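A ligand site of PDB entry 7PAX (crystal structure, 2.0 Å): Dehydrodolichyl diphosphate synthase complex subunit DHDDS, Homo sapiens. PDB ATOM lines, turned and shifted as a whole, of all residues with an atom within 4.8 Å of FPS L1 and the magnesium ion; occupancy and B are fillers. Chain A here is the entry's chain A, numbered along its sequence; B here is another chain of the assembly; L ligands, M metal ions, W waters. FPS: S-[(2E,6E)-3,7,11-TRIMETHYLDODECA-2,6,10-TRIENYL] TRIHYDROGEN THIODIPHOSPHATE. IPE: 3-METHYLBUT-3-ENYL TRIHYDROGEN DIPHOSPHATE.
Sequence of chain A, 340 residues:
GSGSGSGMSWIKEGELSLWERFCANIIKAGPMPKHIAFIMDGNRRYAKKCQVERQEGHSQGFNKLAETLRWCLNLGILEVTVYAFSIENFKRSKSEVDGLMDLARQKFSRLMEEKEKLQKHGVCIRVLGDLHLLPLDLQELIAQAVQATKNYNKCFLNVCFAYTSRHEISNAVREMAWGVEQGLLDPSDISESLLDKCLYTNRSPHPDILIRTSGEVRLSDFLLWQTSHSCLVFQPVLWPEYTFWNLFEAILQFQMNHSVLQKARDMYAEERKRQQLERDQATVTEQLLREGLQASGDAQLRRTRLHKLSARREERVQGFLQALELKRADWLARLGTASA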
ATOM      1  N   TRP A  10      17.682  17.154 -23.727  1.00  0.00           N
ATOM      2  CA  TRP A  10      19.109  17.361 -23.472  1.00  0.00           C
ATOM      3  C   TRP A  10      19.837  18.103 -24.589  1.00  0.00           C
ATOM      4  O   TRP A  10      21.001  18.478 -24.389  1.00  0.00           O
ATOM      5  CB  TRP A  10      19.795  16.014 -23.251  1.00  0.00           C
ATOM      6  CG  TRP A  10      20.647  15.935 -22.011  1.00  0.00           C
ATOM      7  CD1 TRP A  10      22.001  16.011 -21.947  1.00  0.00           C
ATOM      8  CD2 TRP A  10      20.193  15.714 -20.661  1.00  0.00           C
ATOM      9  NE1 TRP A  10      22.429  15.874 -20.648  1.00  0.00           N
ATOM     10  CE2 TRP A  10      21.342  15.687 -19.846  1.00  0.00           C
ATOM     11  CE3 TRP A  10      18.946  15.547 -20.080  1.00  0.00           C
ATOM     12  CZ2 TRP A  10      21.268  15.500 -18.465  1.00  0.00           C
ATOM     13  CZ3 TRP A  10      18.876  15.360 -18.722  1.00  0.00           C
ATOM     14  CH2 TRP A  10      20.020  15.338 -17.926  1.00  0.00           C
ATOM     15  N   MET A  40      29.631  25.715 -15.466  1.00  0.00           N
ATOM     16  CA  MET A  40      28.406  26.441 -15.830  1.00  0.00           C
ATOM     17  C   MET A  40      27.981  27.395 -14.711  1.00  0.00           C
ATOM     18  O   MET A  40      26.982  27.197 -14.020  1.00  0.00           O
ATOM     19  CB  MET A  40      27.288  25.455 -16.157  1.00  0.00           C
ATOM     20  CG  MET A  40      27.665  24.445 -17.227  1.00  0.00           C
ATOM     21  SD  MET A  40      26.326  23.309 -17.628  1.00  0.00           S
ATOM     22  CE  MET A  40      26.086  22.479 -16.062  1.00  0.00           C
ATOM     23  N   ASP A  41      28.743  28.484 -14.584  1.00  0.00           N
ATOM     24  CA  ASP A  41      28.669  29.353 -13.418  1.00  0.00           C
ATOM     25  C   ASP A  41      27.876  30.625 -13.710  1.00  0.00           C
ATOM     26  O   ASP A  41      27.937  31.162 -14.813  1.00  0.00           O
ATOM     27  CB  ASP A  41      30.090  29.730 -12.972  1.00  0.00           C
ATOM     28  CG  ASP A  41      30.138  30.177 -11.522  1.00  0.00           C
ATOM     29  OD1 ASP A  41      29.148  29.955 -10.798  1.00  0.00           O
ATOM     30  OD2 ASP A  41      31.176  30.756 -11.123  1.00  0.00           O
ATOM     31  N   GLY A  42      27.154  31.106 -12.697  1.00  0.00           N
ATOM     32  CA  GLY A  42      26.427  32.357 -12.765  1.00  0.00           C
ATOM     33  C   GLY A  42      24.916  32.240 -12.810  1.00  0.00           C
ATOM     34  O   GLY A  42      24.250  33.271 -13.013  1.00  0.00           O
ATOM     35  N   ASN A  43      24.347  31.044 -12.620  1.00  0.00           N
ATOM     36  CA  ASN A  43      22.901  30.852 -12.716  1.00  0.00           C
ATOM     37  C   ASN A  43      22.145  31.754 -11.752  1.00  0.00           C
ATOM     38  O   ASN A  43      21.098  32.319 -12.102  1.00  0.00           O
ATOM     39  CB  ASN A  43      22.543  29.397 -12.430  1.00  0.00           C
ATOM     40  CG  ASN A  43      23.019  28.449 -13.508  1.00  0.00           C
ATOM     41  OD1 ASN A  43      23.593  28.867 -14.508  1.00  0.00           O
ATOM     42  ND2 ASN A  43      22.782  27.148 -13.305  1.00  0.00           N
ATOM     43  N   ARG A  44      22.633  31.870 -10.512  1.00  0.00           N
ATOM     44  CA  ARG A  44      21.877  32.599  -9.492  1.00  0.00           C
ATOM     45  C   ARG A  44      21.981  34.113  -9.695  1.00  0.00           C
ATOM     46  O   ARG A  44      20.999  34.835  -9.467  1.00  0.00           O
ATOM     47  CB  ARG A  44      22.349  32.197  -8.099  1.00  0.00           C
ATOM     48  CG  ARG A  44      22.112  30.742  -7.759  1.00  0.00           C
ATOM     49  CD  ARG A  44      22.451  30.468  -6.284  1.00  0.00           C
ATOM     50  NE  ARG A  44      23.826  30.828  -5.960  1.00  0.00           N
ATOM     51  CZ  ARG A  44      24.416  30.583  -4.799  1.00  0.00           C
ATOM     52  NH1 ARG A  44      23.740  29.967  -3.831  1.00  0.00           N
ATOM     53  NH2 ARG A  44      25.673  30.946  -4.584  1.00  0.00           N
ATOM     54  N   ARG A  45      23.147  34.603 -10.095  1.00  0.00           N
ATOM     55  CA  ARG A  45      23.244  36.017 -10.433  1.00  0.00           C
ATOM     56  C   ARG A  45      22.366  36.347 -11.625  1.00  0.00           C
ATOM     57  O   ARG A  45      21.702  37.386 -11.642  1.00  0.00           O
ATOM     58  CB  ARG A  45      24.710  36.381 -10.711  1.00  0.00           C
ATOM     59  CG  ARG A  45      25.552  36.567  -9.444  1.00  0.00           C
ATOM     60  CD  ARG A  45      27.038  36.488  -9.750  1.00  0.00           C
ATOM     61  NE  ARG A  45      27.507  35.109  -9.954  1.00  0.00           N
ATOM     62  CZ  ARG A  45      28.748  34.809 -10.328  1.00  0.00           C
ATOM     63  NH1 ARG A  45      29.631  35.774 -10.537  1.00  0.00           N
ATOM     64  NH2 ARG A  45      29.117  33.534 -10.486  1.00  0.00           N
ATOM     65  N   HIS A  58      18.443  28.179 -12.654  1.00  0.00           N
ATOM     66  CA  HIS A  58      19.052  26.868 -12.874  1.00  0.00           C
ATOM     67  C   HIS A  58      18.380  26.131 -14.025  1.00  0.00           C
ATOM     68  O   HIS A  58      19.060  25.458 -14.816  1.00  0.00           O
ATOM     69  CB  HIS A  58      18.977  26.031 -11.599  1.00  0.00           C
ATOM     70  CG  HIS A  58      19.879  26.507 -10.508  1.00  0.00           C
ATOM     71  ND1 HIS A  58      21.215  26.763 -10.710  1.00  0.00           N
ATOM     72  CD2 HIS A  58      19.645  26.770  -9.201  1.00  0.00           C
ATOM     73  CE1 HIS A  58      21.763  27.164  -9.583  1.00  0.00           C
ATOM     74  NE2 HIS A  58      20.830  27.176  -8.643  1.00  0.00           N
ATOM     75  N   GLY A  61      19.675  27.534 -16.969  1.00  0.00           N
ATOM     76  CA  GLY A  61      21.022  27.011 -17.103  1.00  0.00           C
ATOM     77  C   GLY A  61      21.055  25.654 -17.790  1.00  0.00           C
ATOM     78  O   GLY A  61      21.913  25.397 -18.633  1.00  0.00           O
ATOM     79  N   PHE A  62      20.107  24.783 -17.451  1.00  0.00           N
ATOM     80  CA  PHE A  62      20.024  23.510 -18.148  1.00  0.00           C
ATOM     81  C   PHE A  62      19.677  23.699 -19.614  1.00  0.00           C
ATOM     82  O   PHE A  62      20.230  23.021 -20.492  1.00  0.00           O
ATOM     83  CB  PHE A  62      19.000  22.583 -17.483  1.00  0.00           C
ATOM     84  CG  PHE A  62      18.824  21.298 -18.214  1.00  0.00           C
ATOM     85  CD1 PHE A  62      19.683  20.236 -17.985  1.00  0.00           C
ATOM     86  CD2 PHE A  62      17.823  21.151 -19.172  1.00  0.00           C
ATOM     87  CE1 PHE A  62      19.541  19.049 -18.663  1.00  0.00           C
ATOM     88  CE2 PHE A  62      17.679  19.966 -19.860  1.00  0.00           C
ATOM     89  CZ  PHE A  62      18.533  18.907 -19.617  1.00  0.00           C
ATOM     90  N   ALA A  84      28.091  20.282 -13.100  1.00  0.00           N
ATOM     91  CA  ALA A  84      26.674  20.462 -12.813  1.00  0.00           C
ATOM     92  C   ALA A  84      26.354  20.521 -11.329  1.00  0.00           C
ATOM     93  O   ALA A  84      25.398  21.195 -10.940  1.00  0.00           O
ATOM     94  CB  ALA A  84      25.862  19.328 -13.445  1.00  0.00           C
ATOM     95  N   ASN A  89      28.355  22.263  -3.094  1.00  0.00           N
ATOM     96  CA  ASN A  89      27.004  22.802  -3.245  1.00  0.00           C
ATOM     97  C   ASN A  89      25.998  22.148  -2.311  1.00  0.00           C
ATOM     98  O   ASN A  89      24.891  22.668  -2.154  1.00  0.00           O
ATOM     99  CB  ASN A  89      26.527  22.655  -4.691  1.00  0.00           C
ATOM    100  CG  ASN A  89      27.358  23.456  -5.665  1.00  0.00           C
ATOM    101  OD1 ASN A  89      27.614  23.017  -6.783  1.00  0.00           O
ATOM    102  ND2 ASN A  89      27.782  24.641  -5.242  1.00  0.00           N
ATOM    103  N   ARG A  92      24.521  24.520   0.375  1.00  0.00           N
ATOM    104  CA  ARG A  92      23.493  25.515   0.126  1.00  0.00           C
ATOM    105  C   ARG A  92      22.217  25.150   0.881  1.00  0.00           C
ATOM    106  O   ARG A  92      22.104  24.089   1.488  1.00  0.00           O
ATOM    107  CB  ARG A  92      23.227  25.641  -1.379  1.00  0.00           C
ATOM    108  CG  ARG A  92      24.478  26.029  -2.164  1.00  0.00           C
ATOM    109  CD  ARG A  92      24.194  26.284  -3.637  1.00  0.00           C
ATOM    110  NE  ARG A  92      25.388  26.814  -4.322  1.00  0.00           N
ATOM    111  CZ  ARG A  92      25.391  27.305  -5.552  1.00  0.00           C
ATOM    112  NH1 ARG A  92      24.276  27.347  -6.264  1.00  0.00           N
ATOM    113  NH2 ARG A  92      26.519  27.759  -6.083  1.00  0.00           N
ATOM    114  N   GLU A  96      17.254  25.364  -2.049  1.00  0.00           N
ATOM    115  CA  GLU A  96      17.943  25.373  -3.328  1.00  0.00           C
ATOM    116  C   GLU A  96      18.443  23.984  -3.704  1.00  0.00           C
ATOM    117  O   GLU A  96      18.339  23.584  -4.869  1.00  0.00           O
ATOM    118  CB  GLU A  96      19.123  26.360  -3.296  1.00  0.00           C
ATOM    119  CG  GLU A  96      20.027  26.187  -4.511  1.00  0.00           C
ATOM    120  CD  GLU A  96      20.979  27.345  -4.746  1.00  0.00           C
ATOM    121  OE1 GLU A  96      21.116  28.220  -3.858  1.00  0.00           O
ATOM    122  OE2 GLU A  96      21.585  27.367  -5.828  1.00  0.00           O
ATOM    123  N   LEU A 100      17.596  21.825  -7.044  1.00  0.00           N
ATOM    124  CA  LEU A 100      18.543  21.244  -7.993  1.00  0.00           C
ATOM    125  C   LEU A 100      18.334  19.742  -8.136  1.00  0.00           C
ATOM    126  O   LEU A 100      18.318  19.215  -9.253  1.00  0.00           O
ATOM    127  CB  LEU A 100      19.967  21.568  -7.564  1.00  0.00           C
ATOM    128  CG  LEU A 100      20.340  23.031  -7.776  1.00  0.00           C
ATOM    129  CD1 LEU A 100      21.632  23.384  -7.025  1.00  0.00           C
ATOM    130  CD2 LEU A 100      20.475  23.332  -9.267  1.00  0.00           C
ATOM    131  N   LEU A 103      15.322  19.206 -10.262  1.00  0.00           N
ATOM    132  CA  LEU A 103      15.630  19.461 -11.660  1.00  0.00           C
ATOM    133  C   LEU A 103      16.367  18.286 -12.281  1.00  0.00           C
ATOM    134  O   LEU A 103      16.023  17.831 -13.379  1.00  0.00           O
ATOM    135  CB  LEU A 103      16.439  20.752 -11.787  1.00  0.00           C
ATOM    136  CG  LEU A 103      16.731  21.268 -13.191  1.00  0.00           C
ATOM    137  CD1 LEU A 103      15.442  21.535 -13.953  1.00  0.00           C
ATOM    138  CD2 LEU A 103      17.578  22.536 -13.119  1.00  0.00           C
ATOM    139  N   ALA A 104      17.380  17.770 -11.576  1.00  0.00           N
ATOM    140  CA  ALA A 104      18.130  16.627 -12.083  1.00  0.00           C
ATOM    141  C   ALA A 104      17.239  15.397 -12.196  1.00  0.00           C
ATOM    142  O   ALA A 104      17.349  14.624 -13.160  1.00  0.00           O
ATOM    143  CB  ALA A 104      19.327  16.333 -11.187  1.00  0.00           C
ATOM    144  N   LYS A 107      15.138  15.992 -15.380  1.00  0.00           N
ATOM    145  CA  LYS A 107      15.850  15.917 -16.647  1.00  0.00           C
ATOM    146  C   LYS A 107      16.292  14.494 -16.975  1.00  0.00           C
ATOM    147  O   LYS A 107      16.220  14.065 -18.113  1.00  0.00           O
ATOM    148  CB  LYS A 107      17.033  16.866 -16.658  1.00  0.00           C
ATOM    149  CG  LYS A 107      16.637  18.313 -16.582  1.00  0.00           C
ATOM    150  CD  LYS A 107      15.455  18.595 -17.484  1.00  0.00           C
ATOM    151  CE  LYS A 107      15.058  20.058 -17.435  1.00  0.00           C
ATOM    152  NZ  LYS A 107      13.988  20.382 -18.397  1.00  0.00           N
ATOM    153  N   PHE A 108      16.778  13.763 -15.973  1.00  0.00           N
ATOM    154  CA  PHE A 108      17.226  12.387 -16.171  1.00  0.00           C
ATOM    155  C   PHE A 108      16.169  11.355 -16.549  1.00  0.00           C
ATOM    156  O   PHE A 108      16.413  10.485 -17.361  1.00  0.00           O
ATOM    157  CB  PHE A 108      18.000  11.895 -14.958  1.00  0.00           C
ATOM    158  CG  PHE A 108      19.438  12.309 -14.956  1.00  0.00           C
ATOM    159  CD1 PHE A 108      20.343  11.673 -15.761  1.00  0.00           C
ATOM    160  CD2 PHE A 108      19.868  13.341 -14.161  1.00  0.00           C
ATOM    161  CE1 PHE A 108      21.659  12.059 -15.769  1.00  0.00           C
ATOM    162  CE2 PHE A 108      21.186  13.724 -14.159  1.00  0.00           C
ATOM    163  CZ  PHE A 108      22.083  13.083 -14.974  1.00  0.00           C
ATOM    164  N   VAL A 159      28.642  14.430 -17.305  1.00  0.00           N
ATOM    165  CA  VAL A 159      28.027  15.320 -16.338  1.00  0.00           C
ATOM    166  C   VAL A 159      28.695  15.098 -14.996  1.00  0.00           C
ATOM    167  O   VAL A 159      28.665  13.987 -14.447  1.00  0.00           O
ATOM    168  CB  VAL A 159      26.513  15.076 -16.238  1.00  0.00           C
ATOM    169  CG1 VAL A 159      25.900  16.025 -15.222  1.00  0.00           C
ATOM    170  CG2 VAL A 159      25.849  15.244 -17.597  1.00  0.00           C
ATOM    171  N   PHE A 161      28.501  15.478 -11.336  1.00  0.00           N
ATOM    172  CA  PHE A 161      27.429  15.680 -10.369  1.00  0.00           C
ATOM    173  C   PHE A 161      27.858  15.084  -9.033  1.00  0.00           C
ATOM    174  O   PHE A 161      28.307  13.933  -8.972  1.00  0.00           O
ATOM    175  CB  PHE A 161      26.132  15.036 -10.861  1.00  0.00           C
ATOM    176  CG  PHE A 161      24.887  15.807 -10.498  1.00  0.00           C
ATOM    177  CD1 PHE A 161      24.262  15.607  -9.281  1.00  0.00           C
ATOM    178  CD2 PHE A 161      24.318  16.701 -11.398  1.00  0.00           C
ATOM    179  CE1 PHE A 161      23.100  16.313  -8.948  1.00  0.00           C
ATOM    180  CE2 PHE A 161      23.163  17.400 -11.069  1.00  0.00           C
ATOM    181  CZ  PHE A 161      22.555  17.200  -9.846  1.00  0.00           C
ATOM    182  N   ARG A 212      35.138  28.691 -17.939  1.00  0.00           N
ATOM    183  CA  ARG A 212      34.314  29.103 -16.802  1.00  0.00           C
ATOM    184  C   ARG A 212      33.656  30.446 -17.097  1.00  0.00           C
ATOM    185  O   ARG A 212      34.340  31.418 -17.447  1.00  0.00           O
ATOM    186  CB  ARG A 212      35.098  29.191 -15.495  1.00  0.00           C
ATOM    187  CG  ARG A 212      34.184  29.570 -14.323  1.00  0.00           C
ATOM    188  CD  ARG A 212      34.812  29.329 -12.977  1.00  0.00           C
ATOM    189  NE  ARG A 212      33.830  29.421 -11.905  1.00  0.00           N
ATOM    190  CZ  ARG A 212      34.003  28.879 -10.703  1.00  0.00           C
ATOM    191  NH1 ARG A 212      35.118  28.214 -10.443  1.00  0.00           N
ATOM    192  NH2 ARG A 212      33.055  28.982  -9.775  1.00  0.00           N
ATOM    193  N   ARG B 216      32.882  32.295  -2.529  1.00  0.00           N
ATOM    194  CA  ARG B 216      31.649  31.804  -1.929  1.00  0.00           C
ATOM    195  C   ARG B 216      31.749  30.370  -1.433  1.00  0.00           C
ATOM    196  O   ARG B 216      30.889  29.947  -0.651  1.00  0.00           O
ATOM    197  CB  ARG B 216      30.496  31.929  -2.939  1.00  0.00           C
ATOM    198  CG  ARG B 216      30.169  33.381  -3.287  1.00  0.00           C
ATOM    199  CD  ARG B 216      29.061  33.498  -4.332  1.00  0.00           C
ATOM    200  NE  ARG B 216      29.563  33.291  -5.681  1.00  0.00           N
ATOM    201  CZ  ARG B 216      30.181  34.220  -6.402  1.00  0.00           C
ATOM    202  NH1 ARG B 216      30.378  35.427  -5.893  1.00  0.00           N
ATOM    203  NH2 ARG B 216      30.594  33.946  -7.630  1.00  0.00           N
HETATM  204  C1  FPS L   1      26.444  26.682 -10.997  1.00  0.00           C
HETATM  205  S1  FPS L   1      25.832  28.373 -11.254  1.00  0.00           S
HETATM  206  C2  FPS L   1      25.388  25.649 -11.374  1.00  0.00           C
HETATM  207  C3  FPS L   1      24.797  24.916 -10.463  1.00  0.00           C
HETATM  208  C4  FPS L   1      25.145  25.088  -8.987  1.00  0.00           C
HETATM  209  C5  FPS L   1      23.731  23.894 -10.878  1.00  0.00           C
HETATM  210  C6  FPS L   1      23.924  23.550 -12.360  1.00  0.00           C
HETATM  211  C7  FPS L   1      22.594  23.694 -13.094  1.00  0.00           C
HETATM  212  C8  FPS L   1      22.101  22.722 -13.834  1.00  0.00           C
HETATM  213  C10 FPS L   1      22.820  21.381 -14.005  1.00  0.00           C
HETATM  214  C9  FPS L   1      20.776  22.935 -14.528  1.00  0.00           C
HETATM  215  C11 FPS L   1      22.104  20.317 -13.181  1.00  0.00           C
HETATM  216  C12 FPS L   1      21.072  19.535 -13.995  1.00  0.00           C
HETATM  217  C13 FPS L   1      21.393  18.460 -14.684  1.00  0.00           C
HETATM  218  C14 FPS L   1      20.327  17.705 -15.471  1.00  0.00           C
HETATM  219  C15 FPS L   1      22.827  17.922 -14.726  1.00  0.00           C
HETATM  220  PA  FPS L   1      25.498  29.184  -9.330  1.00  0.00           P
HETATM  221  O1A FPS L   1      24.355  28.435  -8.690  1.00  0.00           O
HETATM  222  O2A FPS L   1      26.761  29.013  -8.523  1.00  0.00           O
HETATM  223  O3A FPS L   1      25.080  30.762  -9.510  1.00  0.00           O
HETATM  224  PB  FPS L   1      26.015  32.015  -9.036  1.00  0.00           P
HETATM  225  O1B FPS L   1      25.908  32.157  -7.528  1.00  0.00           O
HETATM  226  O2B FPS L   1      25.479  33.251  -9.694  1.00  0.00           O
HETATM  227  O3B FPS L   1      27.464  31.739  -9.412  1.00  0.00           O
HETATM  228  C1  IPE L   2      31.232  25.280  -9.177  1.00  0.00           C
HETATM  229  O1  IPE L   2      30.684  26.561  -9.035  1.00  0.00           O
HETATM  230  C2  IPE L   2      30.124  24.234  -9.052  1.00  0.00           C
HETATM  231  C3  IPE L   2      29.302  24.084 -10.335  1.00  0.00           C
HETATM  232  C4  IPE L   2      28.344  23.166 -10.414  1.00  0.00           C
HETATM  233  C5  IPE L   2      29.573  25.001 -11.529  1.00  0.00           C
HETATM  234  PA  IPE L   2      30.595  27.275  -7.567  1.00  0.00           P
HETATM  235  O1A IPE L   2      29.743  28.498  -7.623  1.00  0.00           O
HETATM  236  O2A IPE L   2      29.993  26.299  -6.596  1.00  0.00           O
HETATM  237  O3A IPE L   2      32.100  27.726  -7.121  1.00  0.00           O
HETATM  238  PB  IPE L   2      32.458  28.981  -6.134  1.00  0.00           P
HETATM  239  O1B IPE L   2      32.347  30.311  -6.820  1.00  0.00           O
HETATM  240  O2B IPE L   2      31.505  28.977  -4.958  1.00  0.00           O
HETATM  241  O3B IPE L   2      33.881  28.759  -5.672  1.00  0.00           O
HETATM  242 MG    MG M   1      28.652  30.061  -8.772  1.00  0.00          MG
HETATM  243  O   HOH W   1      28.418  30.746  -6.943  1.00  0.00           O
HETATM  244  O   HOH W   2      30.561  31.063  -8.632  1.00  0.00           O
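A sulfur (S1) of FPS L1 sits close to the backbone NH of Gly 42, 3.4 Å away. NH2 of Arg 212 lies within salt-bridge range of O1B of IPE L2 (3.3 Å). The guanidinium group of Arg 92 lies within salt-bridge range of an oxygen (O1A) of FPS L1 (2.7 Å). An oxygen (O3A) of FPS L1 is in hydrogen-bond range of the backbone NH of Asn 43, at 3.2 Å. ND2 of Asn 89 sits at hydrogen-bond distance from O2A of IPE L2, at 3.1 Å. The backbone NH (N) of Arg 44 lies within hydrogen-bond range of an oxygen (O3A) of FPS L1 (2.9 Å). The backbone NH of Arg 45 lies within hydrogen-bond range of an oxygen (O2B) of FPS L1. O2B of FPS L1 lies within salt-bridge range of NE of Arg 45, at 2.8 Å. An oxygen (O1B) of FPS L1 is in salt-bridge range of the guanidinium group (NE) of Arg 44. An oxygen (O2A) of IPE L2 is in salt-bridge range of the guanidinium group of Arg 92 (3.8 Å).
A ring nitrogen (NE2) of His 58 is in hydrogen-bond range of the side-chain carboxylate (OE2) of Glu 96. The guanidinium group of Arg 212 lies within salt-bridge range of the side-chain carboxylate of Asp 41 (2.9 Å). ND2 of Asn 43 sits at hydrogen-bond distance from ND1 of His 58 (3.1 Å). The side-chain amide nitrogen (ND2) of Asn 89 sits close to the guanidinium group (NE) of Arg 92, 3.4 Å away. The guanidinium group (NH1) of Arg 44 is in salt-bridge range of the side-chain carboxylate (OE1) of Glu 96 (3.2 Å). The side-chain carboxylate (OD2) of Asp 41 is in salt-bridge range of the guanidinium group (NH2) of Arg 45 (3.5 Å). The side-chain carboxylate (OE2) of Glu 96 is in salt-bridge range of the guanidinium group (NH1) of Arg 92 (2.7 Å).
O of Met 40 sits close to S1 of FPS L1, at 3.2 Å. Trp 10 touches FPS L1. CE1 of His 58 touches O1A of FPS L1, at 3.0 Å. Phe 62 touches FPS L1. Ala 84 touches FPS L1. OD1 of Asn 89 touches C4 of FPS L1 (3.9 Å). Leu 100 touches FPS L1. CD2 of Leu 103 touches C9 of FPS L1, at 3.5 Å. CB of Lys 107 touches C14 of FPS L1, 3.6 Å away. Val 159 touches FPS L1. CE2 of Phe 161 touches C15 of FPS L1, 3.7 Å away. Hydrophobic or aromatic side chains that line FPS L1: Trp 10, His 58, Phe 62, Ala 84, Leu 100, Leu 103, Val 159 and Phe 161. Within 4 Å of FPS L1: Trp 10, Met 40, Asp 41, Gly 42, Asn 43, Arg 44, Arg 45, His 58, Phe 62, Ala 84, Asn 89, Arg 92, Leu 100, Leu 103, Lys 107, Val 159 and Phe 161. The nearest printed residue that does not touch FPS L1 is Glu 96 (4.1 Å).
Residues that only touch the magnesium ion: Arg 45. Of the 23 residues printed, 2 come within 4 Å of the magnesium ion.
The magnesium ion is bound by water W1 (2.0 Å), OD1 of Asp 41 (2.1 Å), O3B of FPS L1 (2.2 Å), water W2 (2.2 Å), O2A of FPS L1 (2.2 Å) and O1A of IPE L2 (2.2 Å). The magnesium ion has six donor atoms within binding distance.
Water W1 bridges O1B of FPS L1 and NE of Arg 216 of chain B.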
